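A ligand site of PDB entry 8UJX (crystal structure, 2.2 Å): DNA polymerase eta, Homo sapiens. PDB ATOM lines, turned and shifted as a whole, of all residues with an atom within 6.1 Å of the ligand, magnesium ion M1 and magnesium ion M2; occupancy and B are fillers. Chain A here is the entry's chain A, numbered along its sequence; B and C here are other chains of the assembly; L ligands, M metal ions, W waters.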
ATOM      1  N   ASP A  16       0.418  -3.135   8.836  1.00  0.00           N
ATOM      2  CA  ASP A  16       0.643  -4.430   9.460  1.00  0.00           C
ATOM      3  C   ASP A  16      -0.690  -5.103   9.761  1.00  0.00           C
ATOM      4  O   ASP A  16      -1.533  -4.539  10.470  1.00  0.00           O
ATOM      5  CB  ASP A  16       1.474  -4.271  10.722  1.00  0.00           C
ATOM      6  CG  ASP A  16       1.823  -5.571  11.350  1.00  0.00           C
ATOM      7  OD1 ASP A  16       0.935  -6.199  11.948  1.00  0.00           O
ATOM      8  OD2 ASP A  16       2.988  -6.003  11.213  1.00  0.00           O
ATOM      9  N   MET A  17      -0.880  -6.320   9.230  1.00  0.00           N
ATOM     10  CA  MET A  17      -2.143  -7.021   9.392  1.00  0.00           C
ATOM     11  C   MET A  17      -2.403  -7.370  10.852  1.00  0.00           C
ATOM     12  O   MET A  17      -1.479  -7.747  11.591  1.00  0.00           O
ATOM     13  CB  MET A  17      -2.165  -8.292   8.529  1.00  0.00           C
ATOM     14  CG  MET A  17      -1.762  -8.087   7.055  1.00  0.00           C
ATOM     15  SD  MET A  17      -2.720  -6.832   6.167  1.00  0.00           S
ATOM     16  CE  MET A  17      -4.332  -7.547   6.291  1.00  0.00           C
ATOM     17  N   ASP A  18      -3.637  -7.207  11.288  1.00  0.00           N
ATOM     18  CA  ASP A  18      -4.009  -7.572  12.652  1.00  0.00           C
ATOM     19  C   ASP A  18      -4.131  -9.088  12.740  1.00  0.00           C
ATOM     20  O   ASP A  18      -4.707  -9.718  11.851  1.00  0.00           O
ATOM     21  CB  ASP A  18      -5.325  -6.911  13.059  1.00  0.00           C
ATOM     22  CG  ASP A  18      -5.293  -5.380  12.926  1.00  0.00           C
ATOM     23  OD1 ASP A  18      -4.218  -4.780  13.067  1.00  0.00           O
ATOM     24  OD2 ASP A  18      -6.367  -4.786  12.686  1.00  0.00           O
ATOM     25  N   CYS A  19      -3.617  -9.648  13.837  1.00  0.00           N
ATOM     26  CA  CYS A  19      -3.504 -11.079  14.103  1.00  0.00           C
ATOM     27  C   CYS A  19      -3.586 -11.905  12.826  1.00  0.00           C
ATOM     28  O   CYS A  19      -4.566 -12.615  12.587  1.00  0.00           O
ATOM     29  CB  CYS A  19      -4.579 -11.514  15.125  1.00  0.00           C
ATOM     30  SG  CYS A  19      -6.317 -11.002  14.793  1.00  0.00           S
ATOM     31  N   PHE A  20      -2.551 -11.820  11.979  1.00  0.00           N
ATOM     32  CA  PHE A  20      -2.708 -12.161  10.568  1.00  0.00           C
ATOM     33  C   PHE A  20      -3.094 -13.629  10.345  1.00  0.00           C
ATOM     34  O   PHE A  20      -4.036 -13.927   9.602  1.00  0.00           O
ATOM     35  CB  PHE A  20      -1.425 -11.808   9.827  1.00  0.00           C
ATOM     36  CG  PHE A  20      -1.514 -12.050   8.360  1.00  0.00           C
ATOM     37  CD1 PHE A  20      -2.619 -11.609   7.638  1.00  0.00           C
ATOM     38  CD2 PHE A  20      -0.526 -12.756   7.710  1.00  0.00           C
ATOM     39  CE1 PHE A  20      -2.722 -11.859   6.271  1.00  0.00           C
ATOM     40  CE2 PHE A  20      -0.619 -13.013   6.335  1.00  0.00           C
ATOM     41  CZ  PHE A  20      -1.713 -12.573   5.626  1.00  0.00           C
ATOM     42  N   PHE A  21      -2.368 -14.569  10.956  1.00  0.00           N
ATOM     43  CA  PHE A  21      -2.681 -15.965  10.656  1.00  0.00           C
ATOM     44  C   PHE A  21      -4.085 -16.343  11.152  1.00  0.00           C
ATOM     45  O   PHE A  21      -4.778 -17.117  10.498  1.00  0.00           O
ATOM     46  CB  PHE A  21      -1.637 -16.903  11.263  1.00  0.00           C
ATOM     47  CG  PHE A  21      -0.291 -16.892  10.561  1.00  0.00           C
ATOM     48  CD1 PHE A  21       0.132 -15.817   9.809  1.00  0.00           C
ATOM     49  CD2 PHE A  21       0.569 -17.974  10.707  1.00  0.00           C
ATOM     50  CE1 PHE A  21       1.383 -15.815   9.184  1.00  0.00           C
ATOM     51  CE2 PHE A  21       1.825 -17.994  10.091  1.00  0.00           C
ATOM     52  CZ  PHE A  21       2.236 -16.904   9.326  1.00  0.00           C
ATOM     53  N   VAL A  22      -4.515 -15.769  12.293  1.00  0.00           N
ATOM     54  CA  VAL A  22      -5.888 -15.961  12.782  1.00  0.00           C
ATOM     55  C   VAL A  22      -6.909 -15.464  11.766  1.00  0.00           C
ATOM     56  O   VAL A  22      -7.882 -16.153  11.447  1.00  0.00           O
ATOM     57  CB  VAL A  22      -6.047 -15.257  14.158  1.00  0.00           C
ATOM     58  CG1 VAL A  22      -7.479 -15.205  14.591  1.00  0.00           C
ATOM     59  CG2 VAL A  22      -5.237 -15.989  15.198  1.00  0.00           C
ATOM     60  N   GLN A  41       1.271 -24.361  16.031  1.00  0.00           N
ATOM     61  CA  GLN A  41       2.107 -25.297  15.275  1.00  0.00           C
ATOM     62  C   GLN A  41       2.256 -26.589  16.087  1.00  0.00           C
ATOM     63  O   GLN A  41       2.621 -26.542  17.259  1.00  0.00           O
ATOM     64  CB  GLN A  41       3.492 -24.715  14.970  1.00  0.00           C
ATOM     65  CG  GLN A  41       3.471 -23.522  14.019  1.00  0.00           C
ATOM     66  CD  GLN A  41       4.851 -23.048  13.557  1.00  0.00           C
ATOM     67  OE1 GLN A  41       5.133 -23.025  12.356  1.00  0.00           O
ATOM     68  NE2 GLN A  41       5.684 -22.621  14.500  1.00  0.00           N
ATOM     69  N   ILE A  51       1.395 -19.249  17.670  1.00  0.00           N
ATOM     70  CA  ILE A  51       2.093 -18.172  16.986  1.00  0.00           C
ATOM     71  C   ILE A  51       1.207 -16.982  16.645  1.00  0.00           C
ATOM     72  O   ILE A  51       1.730 -15.950  16.188  1.00  0.00           O
ATOM     73  CB  ILE A  51       2.823 -18.670  15.718  1.00  0.00           C
ATOM     74  CG1 ILE A  51       1.824 -19.156  14.660  1.00  0.00           C
ATOM     75  CG2 ILE A  51       3.865 -19.743  16.073  1.00  0.00           C
ATOM     76  CD1 ILE A  51       2.493 -19.577  13.371  1.00  0.00           C
ATOM     77  N   ALA A  52      -0.114 -17.064  16.847  1.00  0.00           N
ATOM     78  CA  ALA A  52      -0.977 -15.923  16.581  1.00  0.00           C
ATOM     79  C   ALA A  52      -2.255 -16.027  17.408  1.00  0.00           C
ATOM     80  O   ALA A  52      -2.782 -17.129  17.596  1.00  0.00           O
ATOM     81  CB  ALA A  52      -1.323 -15.828  15.082  1.00  0.00           C
ATOM     82  N   VAL A  53      -2.761 -14.888  17.880  1.00  0.00           N
ATOM     83  CA  VAL A  53      -3.795 -14.853  18.904  1.00  0.00           C
ATOM     84  C   VAL A  53      -4.805 -13.778  18.538  1.00  0.00           C
ATOM     85  O   VAL A  53      -4.427 -12.610  18.356  1.00  0.00           O
ATOM     86  CB  VAL A  53      -3.194 -14.555  20.302  1.00  0.00           C
ATOM     87  CG1 VAL A  53      -4.280 -14.576  21.380  1.00  0.00           C
ATOM     88  CG2 VAL A  53      -2.077 -15.503  20.627  1.00  0.00           C
ATOM     89  N   TYR A  55      -7.741 -10.963  19.130  1.00  0.00           N
ATOM     90  CA  TYR A  55      -7.824  -9.969  20.210  1.00  0.00           C
ATOM     91  C   TYR A  55      -8.784 -10.400  21.317  1.00  0.00           C
ATOM     92  O   TYR A  55      -8.554 -10.102  22.495  1.00  0.00           O
ATOM     93  CB  TYR A  55      -8.166  -8.582  19.634  1.00  0.00           C
ATOM     94  CG  TYR A  55      -6.926  -7.935  19.012  1.00  0.00           C
ATOM     95  CD1 TYR A  55      -6.454  -8.358  17.772  1.00  0.00           C
ATOM     96  CD2 TYR A  55      -6.219  -6.934  19.669  1.00  0.00           C
ATOM     97  CE1 TYR A  55      -5.308  -7.810  17.198  1.00  0.00           C
ATOM     98  CE2 TYR A  55      -5.057  -6.371  19.091  1.00  0.00           C
ATOM     99  CZ  TYR A  55      -4.615  -6.809  17.851  1.00  0.00           C
ATOM    100  OH  TYR A  55      -3.471  -6.286  17.232  1.00  0.00           O
ATOM    101  N   ARG A  58      -6.536 -12.463  23.468  1.00  0.00           N
ATOM    102  CA  ARG A  58      -5.516 -11.683  24.163  1.00  0.00           C
ATOM    103  C   ARG A  58      -6.023 -11.134  25.499  1.00  0.00           C
ATOM    104  O   ARG A  58      -5.273 -11.068  26.479  1.00  0.00           O
ATOM    105  CB  ARG A  58      -5.030 -10.545  23.267  1.00  0.00           C
ATOM    106  CG  ARG A  58      -4.349 -11.008  21.989  1.00  0.00           C
ATOM    107  CD  ARG A  58      -3.605  -9.877  21.270  1.00  0.00           C
ATOM    108  NE  ARG A  58      -3.340 -10.208  19.875  1.00  0.00           N
ATOM    109  CZ  ARG A  58      -2.627  -9.458  19.040  1.00  0.00           C
ATOM    110  NH1 ARG A  58      -2.114  -8.304  19.416  1.00  0.00           N
ATOM    111  NH2 ARG A  58      -2.435  -9.889  17.802  1.00  0.00           N
ATOM    112  N   ARG A  64       1.549 -15.222  22.037  1.00  0.00           N
ATOM    113  CA  ARG A  64       2.523 -15.907  21.207  1.00  0.00           C
ATOM    114  C   ARG A  64       3.562 -16.617  22.063  1.00  0.00           C
ATOM    115  O   ARG A  64       3.974 -16.104  23.114  1.00  0.00           O
ATOM    116  CB  ARG A  64       3.198 -14.882  20.292  1.00  0.00           C
ATOM    117  CG  ARG A  64       4.358 -15.393  19.479  1.00  0.00           C
ATOM    118  CD  ARG A  64       5.009 -14.247  18.725  1.00  0.00           C
ATOM    119  NE  ARG A  64       6.241 -14.707  18.094  1.00  0.00           N
ATOM    120  CZ  ARG A  64       7.451 -14.554  18.619  1.00  0.00           C
ATOM    121  NH1 ARG A  64       7.650 -13.845  19.721  1.00  0.00           N
ATOM    122  NH2 ARG A  64       8.490 -15.143  18.025  1.00  0.00           N
ATOM    123  N   SER A  65       3.980 -17.796  21.615  1.00  0.00           N
ATOM    124  CA  SER A  65       4.954 -18.682  22.260  1.00  0.00           C
ATOM    125  C   SER A  65       4.392 -19.361  23.499  1.00  0.00           C
ATOM    126  O   SER A  65       5.126 -20.032  24.210  1.00  0.00           O
ATOM    127  CB  SER A  65       6.258 -17.981  22.631  1.00  0.00           C
ATOM    128  OG  SER A  65       7.032 -17.686  21.480  1.00  0.00           O
ATOM    129  N   ALA A  90       6.110 -27.842   9.501  1.00  0.00           N
ATOM    130  CA  ALA A  90       5.231 -26.721   9.218  1.00  0.00           C
ATOM    131  C   ALA A  90       5.199 -26.413   7.724  1.00  0.00           C
ATOM    132  O   ALA A  90       6.214 -26.504   7.023  1.00  0.00           O
ATOM    133  CB  ALA A  90       5.692 -25.488   9.983  1.00  0.00           C
ATOM    134  N   LEU A  92       3.705 -23.195   5.590  1.00  0.00           N
ATOM    135  CA  LEU A  92       3.101 -21.884   5.757  1.00  0.00           C
ATOM    136  C   LEU A  92       2.505 -21.345   4.458  1.00  0.00           C
ATOM    137  O   LEU A  92       2.226 -20.145   4.363  1.00  0.00           O
ATOM    138  CB  LEU A  92       4.126 -20.896   6.326  1.00  0.00           C
ATOM    139  CG  LEU A  92       4.768 -21.262   7.696  1.00  0.00           C
ATOM    140  CD1 LEU A  92       5.790 -20.200   8.146  1.00  0.00           C
ATOM    141  CD2 LEU A  92       3.718 -21.459   8.778  1.00  0.00           C
ATOM    142  N   SER A 116       7.758  -8.111   6.333  1.00  0.00           N
ATOM    143  CA  SER A 116       7.584  -9.466   6.859  1.00  0.00           C
ATOM    144  C   SER A 116       6.451 -10.106   6.072  1.00  0.00           C
ATOM    145  O   SER A 116       5.944  -9.528   5.104  1.00  0.00           O
ATOM    146  CB  SER A 116       7.289  -9.444   8.364  1.00  0.00           C
ATOM    147  OG  SER A 116       5.939  -9.052   8.580  1.00  0.00           O
ATOM    148  N   ILE A 117       6.018 -11.296   6.498  1.00  0.00           N
ATOM    149  CA  ILE A 117       4.909 -11.946   5.832  1.00  0.00           C
ATOM    150  C   ILE A 117       3.632 -11.117   5.941  1.00  0.00           C
ATOM    151  O   ILE A 117       2.730 -11.264   5.108  1.00  0.00           O
ATOM    152  CB  ILE A 117       4.683 -13.376   6.388  1.00  0.00           C
ATOM    153  CG1 ILE A 117       3.857 -14.203   5.400  1.00  0.00           C
ATOM    154  CG2 ILE A 117       3.989 -13.323   7.740  1.00  0.00           C
ATOM    155  CD1 ILE A 117       3.804 -15.697   5.760  1.00  0.00           C
ATOM    156  N   ASP A 118       3.531 -10.230   6.933  1.00  0.00           N
ATOM    157  CA  ASP A 118       2.279  -9.520   7.111  1.00  0.00           C
ATOM    158  C   ASP A 118       2.429  -8.012   7.208  1.00  0.00           C
ATOM    159  O   ASP A 118       1.465  -7.332   7.591  1.00  0.00           O
ATOM    160  CB  ASP A 118       1.534 -10.055   8.343  1.00  0.00           C
ATOM    161  CG  ASP A 118       1.863  -9.285   9.603  1.00  0.00           C
ATOM    162  OD1 ASP A 118       3.064  -9.053   9.850  1.00  0.00           O
ATOM    163  OD2 ASP A 118       0.917  -8.904  10.340  1.00  0.00           O
ATOM    164  N   GLU A 119       3.571  -7.440   6.854  1.00  0.00           N
ATOM    165  CA  GLU A 119       3.638  -5.990   6.860  1.00  0.00           C
ATOM    166  C   GLU A 119       4.570  -5.498   5.771  1.00  0.00           C
ATOM    167  O   GLU A 119       5.459  -6.214   5.290  1.00  0.00           O
ATOM    168  CB  GLU A 119       4.081  -5.445   8.214  1.00  0.00           C
ATOM    169  CG  GLU A 119       5.517  -5.613   8.492  1.00  0.00           C
ATOM    170  CD  GLU A 119       5.767  -5.912   9.944  1.00  0.00           C
ATOM    171  OE1 GLU A 119       5.440  -7.037  10.385  1.00  0.00           O
ATOM    172  OE2 GLU A 119       6.269  -5.020  10.648  1.00  0.00           O
ATOM    173  N   LYS A 227       6.385   2.631  11.974  1.00  0.00           N
ATOM    174  CA  LYS A 227       6.198   1.348  12.650  1.00  0.00           C
ATOM    175  C   LYS A 227       5.756   1.542  14.097  1.00  0.00           C
ATOM    176  O   LYS A 227       4.856   0.852  14.582  1.00  0.00           O
ATOM    177  CB  LYS A 227       7.490   0.511  12.564  1.00  0.00           C
ATOM    178  CG  LYS A 227       7.500  -0.800  13.397  1.00  0.00           C
ATOM    179  CD  LYS A 227       6.822  -1.972  12.670  1.00  0.00           C
ATOM    180  CE  LYS A 227       6.512  -3.167  13.621  1.00  0.00           C
ATOM    181  NZ  LYS A 227       5.843  -4.359  12.967  1.00  0.00           N
ATOM    182  N   LYS A 234      -3.545  -0.293  17.361  1.00  0.00           N
ATOM    183  CA  LYS A 234      -4.010  -1.606  16.943  1.00  0.00           C
ATOM    184  C   LYS A 234      -5.177  -2.031  17.825  1.00  0.00           C
ATOM    185  O   LYS A 234      -5.155  -1.762  19.035  1.00  0.00           O
ATOM    186  CB  LYS A 234      -2.872  -2.628  17.068  1.00  0.00           C
ATOM    187  CG  LYS A 234      -2.048  -2.800  15.826  1.00  0.00           C
ATOM    188  CD  LYS A 234      -1.107  -4.010  15.920  1.00  0.00           C
ATOM    189  CE  LYS A 234      -0.499  -4.367  14.536  1.00  0.00           C
ATOM    190  NZ  LYS A 234      -1.505  -4.992  13.609  1.00  0.00           N
ATOM    191  N   PRO A 235      -6.200  -2.725  17.294  1.00  0.00           N
ATOM    192  CA  PRO A 235      -6.401  -3.190  15.911  1.00  0.00           C
ATOM    193  C   PRO A 235      -7.339  -2.350  15.063  1.00  0.00           C
ATOM    194  O   PRO A 235      -8.127  -1.579  15.599  1.00  0.00           O
ATOM    195  CB  PRO A 235      -7.010  -4.581  16.133  1.00  0.00           C
ATOM    196  CG  PRO A 235      -7.930  -4.343  17.323  1.00  0.00           C
ATOM    197  CD  PRO A 235      -7.155  -3.374  18.205  1.00  0.00           C
ATOM    198  P    DT B   8       9.068  -7.020  15.466  1.00  0.00           P
ATOM    199  OP1  DT B   8       8.230  -5.808  15.297  1.00  0.00           O
ATOM    200  OP2  DT B   8       9.301  -7.615  16.803  1.00  0.00           O
ATOM    201  O5'  DT B   8       8.440  -8.110  14.458  1.00  0.00           O
ATOM    202  C5'  DT B   8       8.470  -7.875  13.006  1.00  0.00           C
ATOM    203  C4'  DT B   8       7.810  -9.017  12.265  1.00  0.00           C
ATOM    204  O4'  DT B   8       8.620 -10.220  12.407  1.00  0.00           O
ATOM    205  C3'  DT B   8       6.424  -9.355  12.801  1.00  0.00           C
ATOM    206  O3'  DT B   8       5.480  -9.538  11.702  1.00  0.00           O
ATOM    207  C2'  DT B   8       6.655 -10.646  13.636  1.00  0.00           C
ATOM    208  C1'  DT B   8       7.853 -11.280  12.948  1.00  0.00           C
ATOM    209  N1   DT B   8       8.736 -12.134  13.861  1.00  0.00           N
ATOM    210  C2   DT B   8       9.042 -13.428  13.475  1.00  0.00           C
ATOM    211  O2   DT B   8       8.649 -13.905  12.433  1.00  0.00           O
ATOM    212  N3   DT B   8       9.833 -14.125  14.346  1.00  0.00           N
ATOM    213  C4   DT B   8      10.348 -13.679  15.555  1.00  0.00           C
ATOM    214  O4   DT B   8      11.064 -14.380  16.279  1.00  0.00           O
ATOM    215  C5   DT B   8       9.984 -12.320  15.910  1.00  0.00           C
ATOM    216  C7   DT B   8      10.485 -11.732  17.191  1.00  0.00           C
ATOM    217  C6   DT B   8       9.204 -11.624  15.053  1.00  0.00           C
ATOM    218  N2  XB9 C   4       9.654 -19.161  16.882  1.00  0.00           N
ATOM    219  N1  XB9 C   4       9.654 -21.442  16.653  1.00  0.00           N
ATOM    220  C2  XB9 C   4       9.157 -20.249  16.318  1.00  0.00           C
ATOM    221  O1  XB9 C   4       8.249 -20.185  15.503  1.00  0.00           O
ATOM    222  C1' XB9 C   4       9.085 -22.636  16.059  1.00  0.00           C
ATOM    223  C2' XB9 C   4      10.253 -23.547  15.713  1.00  0.00           C
ATOM    224  C3' XB9 C   4       9.723 -24.943  16.019  1.00  0.00           C
ATOM    225  C4' XB9 C   4       8.577 -24.744  16.996  1.00  0.00           C
ATOM    226  C5' XB9 C   4       8.904 -25.277  18.386  1.00  0.00           C
ATOM    227  O3' XB9 C   4       9.105 -25.496  14.865  1.00  0.00           O
ATOM    228  O4' XB9 C   4       8.303 -23.342  17.036  1.00  0.00           O
ATOM    229  O5' XB9 C   4      10.267 -24.949  18.657  1.00  0.00           O
ATOM    230  OP1 XB9 C   4      12.086 -23.668  19.896  1.00  0.00           O
ATOM    231  P   XB9 C   4      10.753 -24.379  20.068  1.00  0.00           P
ATOM    232  O2  XB9 C   4      10.805 -25.519  21.064  1.00  0.00           O
ATOM    233  P    DA C   5       9.905 -25.757  13.503  1.00  0.00           P
ATOM    234  OP1  DA C   5       9.171 -26.858  12.839  1.00  0.00           O
ATOM    235  OP2  DA C   5      11.366 -25.888  13.770  1.00  0.00           O
ATOM    236  O5'  DA C   5       9.639 -24.464  12.637  1.00  0.00           O
ATOM    237  C5'  DA C   5       8.353 -24.280  12.039  1.00  0.00           C
ATOM    238  C4'  DA C   5       8.328 -23.063  11.151  1.00  0.00           C
ATOM    239  O4'  DA C   5       8.622 -21.879  11.938  1.00  0.00           O
ATOM    240  C3'  DA C   5       9.324 -23.089  10.002  1.00  0.00           C
ATOM    241  O3'  DA C   5       8.697 -22.607   8.866  1.00  0.00           O
ATOM    242  C2'  DA C   5      10.430 -22.125  10.467  1.00  0.00           C
ATOM    243  C1'  DA C   5       9.633 -21.123  11.292  1.00  0.00           C
ATOM    244  N9   DA C   5      10.405 -20.465  12.343  1.00  0.00           N
ATOM    245  C8   DA C   5      11.286 -21.045  13.208  1.00  0.00           C
ATOM    246  N7   DA C   5      11.807 -20.216  14.079  1.00  0.00           N
ATOM    247  C5   DA C   5      11.223 -18.992  13.764  1.00  0.00           C
ATOM    248  C6   DA C   5      11.362 -17.693  14.319  1.00  0.00           C
ATOM    249  N6   DA C   5      12.165 -17.423  15.343  1.00  0.00           N
ATOM    250  N1   DA C   5      10.631 -16.702  13.774  1.00  0.00           N
ATOM    251  C2   DA C   5       9.815 -16.987  12.744  1.00  0.00           C
ATOM    252  N3   DA C   5       9.602 -18.170  12.137  1.00  0.00           N
ATOM    253  C4   DA C   5      10.343 -19.133  12.698  1.00  0.00           C
ATOM    254  P    DT C   6       9.399 -22.780   7.432  1.00  0.00           P
ATOM    255  OP1  DT C   6       8.322 -22.592   6.434  1.00  0.00           O
ATOM    256  OP2  DT C   6      10.174 -24.031   7.361  1.00  0.00           O
ATOM    257  O5'  DT C   6      10.268 -21.463   7.330  1.00  0.00           O
ATOM    258  C5'  DT C   6       9.564 -20.220   7.515  1.00  0.00           C
ATOM    259  C4'  DT C   6      10.495 -19.051   7.510  1.00  0.00           C
ATOM    260  O4'  DT C   6      10.947 -18.768   8.864  1.00  0.00           O
ATOM    261  C3'  DT C   6      11.758 -19.237   6.662  1.00  0.00           C
ATOM    262  O3'  DT C   6      11.975 -18.101   5.805  1.00  0.00           O
ATOM    263  C2'  DT C   6      12.849 -19.296   7.739  1.00  0.00           C
ATOM    264  C1'  DT C   6      12.251 -18.318   8.743  1.00  0.00           C
ATOM    265  N1   DT C   6      12.940 -18.275  10.070  1.00  0.00           N
ATOM    266  C2   DT C   6      12.887 -17.117  10.808  1.00  0.00           C
ATOM    267  O2   DT C   6      12.258 -16.132  10.448  1.00  0.00           O
ATOM    268  N3   DT C   6      13.575 -17.146  11.981  1.00  0.00           N
ATOM    269  C4   DT C   6      14.309 -18.197  12.490  1.00  0.00           C
ATOM    270  O4   DT C   6      14.885 -18.130  13.568  1.00  0.00           O
ATOM    271  C5   DT C   6      14.337 -19.384  11.659  1.00  0.00           C
ATOM    272  C7   DT C   6      15.097 -20.607  12.108  1.00  0.00           C
ATOM    273  C6   DT C   6      13.669 -19.361  10.491  1.00  0.00           C
HETATM  274  N1  LIG L   1       6.973 -18.524  14.228  1.00  0.00           N
HETATM  275  C1  LIG L   1       6.132 -18.685  13.077  1.00  0.00           C
HETATM  276  N2  LIG L   1       6.171 -19.919  12.308  1.00  0.00           N
HETATM  277  N3  LIG L   1       5.221 -17.614  12.697  1.00  0.00           N
HETATM  278  C2  LIG L   1       5.186 -16.369  13.500  1.00  0.00           C
HETATM  279  C3  LIG L   1       5.989 -16.188  14.579  1.00  0.00           C
HETATM  280  C4  LIG L   1       6.930 -17.310  14.984  1.00  0.00           C
HETATM  281  O1  LIG L   1       7.631 -17.157  15.928  1.00  0.00           O
HETATM  282  N4  LIG L   1       5.741 -14.982  15.099  1.00  0.00           N
HETATM  283  C5  LIG L   1       4.795 -14.390  14.331  1.00  0.00           C
HETATM  284  N5  LIG L   1       4.467 -15.276  13.354  1.00  0.00           N
HETATM  285  P1  LIG L   1       2.869 -10.164  13.836  1.00  0.00           P
HETATM  286  P2  LIG L   1       0.004 -10.636  14.378  1.00  0.00           P
HETATM  287  P3  LIG L   1      -0.720  -8.052  15.494  1.00  0.00           P
HETATM  288  C6  LIG L   1       3.509 -15.226  12.272  1.00  0.00           C
HETATM  289  O2  LIG L   1       2.329  -9.010  13.006  1.00  0.00           O
HETATM  290  O3  LIG L   1      -0.541 -12.019  14.608  1.00  0.00           O
HETATM  291  O4  LIG L   1      -2.131  -7.542  15.380  1.00  0.00           O
HETATM  292  C7  LIG L   1       2.253 -15.278  12.735  1.00  0.00           C
HETATM  293  O5  LIG L   1       4.014  -9.809  14.716  1.00  0.00           O
HETATM  294  O6  LIG L   1      -0.076 -10.164  12.948  1.00  0.00           O
HETATM  295  O7  LIG L   1       0.110  -7.648  14.326  1.00  0.00           O
HETATM  296  C8  LIG L   1       1.709 -13.749  12.689  1.00  0.00           C
HETATM  297  O8  LIG L   1       0.269 -13.718  12.607  1.00  0.00           O
HETATM  298  N6  LIG L   1       1.633 -10.669  14.879  1.00  0.00           N
HETATM  299  O9  LIG L   1      -0.812  -9.681  15.423  1.00  0.00           O
HETATM  300  O10 LIG L   1      -0.120  -7.708  16.843  1.00  0.00           O
HETATM  301  C9  LIG L   1       2.301 -13.200  11.582  1.00  0.00           C
HETATM  302  O11 LIG L   1       3.682 -13.860  11.517  1.00  0.00           O
HETATM  303  C10 LIG L   1       2.551 -11.700  11.717  1.00  0.00           C
HETATM  304  O12 LIG L   1       3.292 -11.436  12.880  1.00  0.00           O
HETATM  305 MG    MG M   1       0.432  -8.262  12.348  1.00  0.00          MG
HETATM  306 MG    MG M   2       3.881  -7.947  11.592  1.00  0.00          MG
HETATM  307  O   HOH W   1       5.837 -12.272  10.897  1.00  0.00           O
HETATM  308  O   HOH W   2       1.586  -9.118  18.232  1.00  0.00           O
HETATM  309  O   HOH W   3       2.252 -13.063  16.642  1.00  0.00           O
HETATM  310  O   HOH W   4       4.234  -7.102  13.491  1.00  0.00           O
HETATM  311  O   HOH W   5      -1.019 -12.584  16.967  1.00  0.00           O
HETATM  312  O   HOH W   6       6.560 -18.517  18.859  1.00  0.00           O
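The side-chain amide oxygen (OE1) of Gln 41 lies within hydrogen-bond range of a nitrogen (N2) of the ligand (3.3 Å). NH1 of Arg 58 lies within salt-bridge range of O10 of the ligand. N of Phe 20 lies within hydrogen-bond range of O3 of the ligand (3.3 Å). N3 of DA 5 of chain C is in hydrogen-bond range of N1 of the ligand. OH of Tyr 55 sits at hydrogen-bond distance from O4 of the ligand (2.6 Å). An oxygen (O4) of the ligand sits at hydrogen-bond distance from the backbone NH (N) of Cys 19. An oxygen (O1) of the ligand is in hydrogen-bond range of the guanidinium group (NH2) of Arg 64, 3.0 Å away. The backbone NH of Phe 21 is in hydrogen-bond range of an oxygen (O8) of the ligand, 3.2 Å away. O4' of DA 5 of chain C is in hydrogen-bond range of N2 of the ligand (3.2 Å). O4 of the ligand lies within salt-bridge range of NZ of Lys 234, 3.2 Å away. A nitrogen (N1) of the ligand is in hydrogen-bond range of O1 of XB9 4 of chain C, at 2.5 Å.
The side-chain carboxylate (OD1) of Asp 18 lies within salt-bridge range of the side-chain amino group (NZ) of Lys 234. The side-chain carboxylate (OD2) of Asp 16 lies close to the side-chain amino group (NZ) of Lys 227. The side-chain hydroxyl (OH) of Tyr 55 lies within hydrogen-bond range of the guanidinium group (NH1) of Arg 58, 3.3 Å away. OE2 of Glu 119 lies within salt-bridge range of NZ of Lys 227. O3' of DT 8 of chain B sits close to the side-chain hydroxyl (OG) of Ser 116, 3.2 Å away. NZ of Lys 234 is in hydrogen-bond range of O of Asp 16. The guanidinium group of Arg 58 is in hydrogen-bond range of the backbone carbonyl oxygen of Val 53 (3.0 Å). NZ of Lys 227 is in salt-bridge range of OP1 of DT 8 of chain B, at 3.6 Å.
Asp 18 touches the ligand (CA to O4, 3.3 Å). Ile 51 touches the ligand (CD1 to N3, 3.4 Å). Ala 52 touches the ligand. CG2 of Ile 117 touches O11 of the ligand, at 3.8 Å. Hydrophobic or aromatic side chains within 4 Å of the ligand: Phe 20, Phe 21, Ile 51, Ala 52, Tyr 55 and Ile 117. The nearest printed residue that does not touch the ligand is Leu 92 (4.2 Å).
Of the 28 residues printed, 3 come within 4 Å of magnesium ion M1.
Ser 116 touches magnesium ion M2 (OG to MG, 3.8 Å). The nearest printed residue that does not touch magnesium ion M2 is Lys 227 (4.3 Å).
Magnesium ion M1 is bound by O6 of the ligand (2.1 Å), O7 of the ligand (2.1 Å), O of Met 17 (2.1 Å), O2 of the ligand (2.1 Å), OD1 of Asp 16 (2.2 Å) and OD2 of Asp 118 (2.2 Å).
Magnesium ion M2 is bound by water W4 (2.1 Å), the side-chain carboxylate (OE1) of Glu 119 (2.2 Å), the side-chain carboxylate (OD2) of Asp 16 (2.2 Å), the side-chain carboxylate (OD1) of Asp 118 (2.2 Å), O3' of DT 8 of chain B (2.3 Å) and an oxygen (O2) of the ligand (2.4 Å).
Water W4 lies within hydrogen-bond range of O5 of the ligand (3.0 Å) and NZ of Lys 227 (3.2 Å). Water W5 lies within hydrogen-bond range of O3 of the ligand, N of Val 53 and NH2 of Arg 58. Water W3 bridges O of Ile 51 (3.0 Å) and N6 of the ligand (3.0 Å). Water W6 bridges the side-chain hydroxyl (OG) of Ser 65 (2.8 Å) and an oxygen (O1) of the ligand (3.4 Å).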
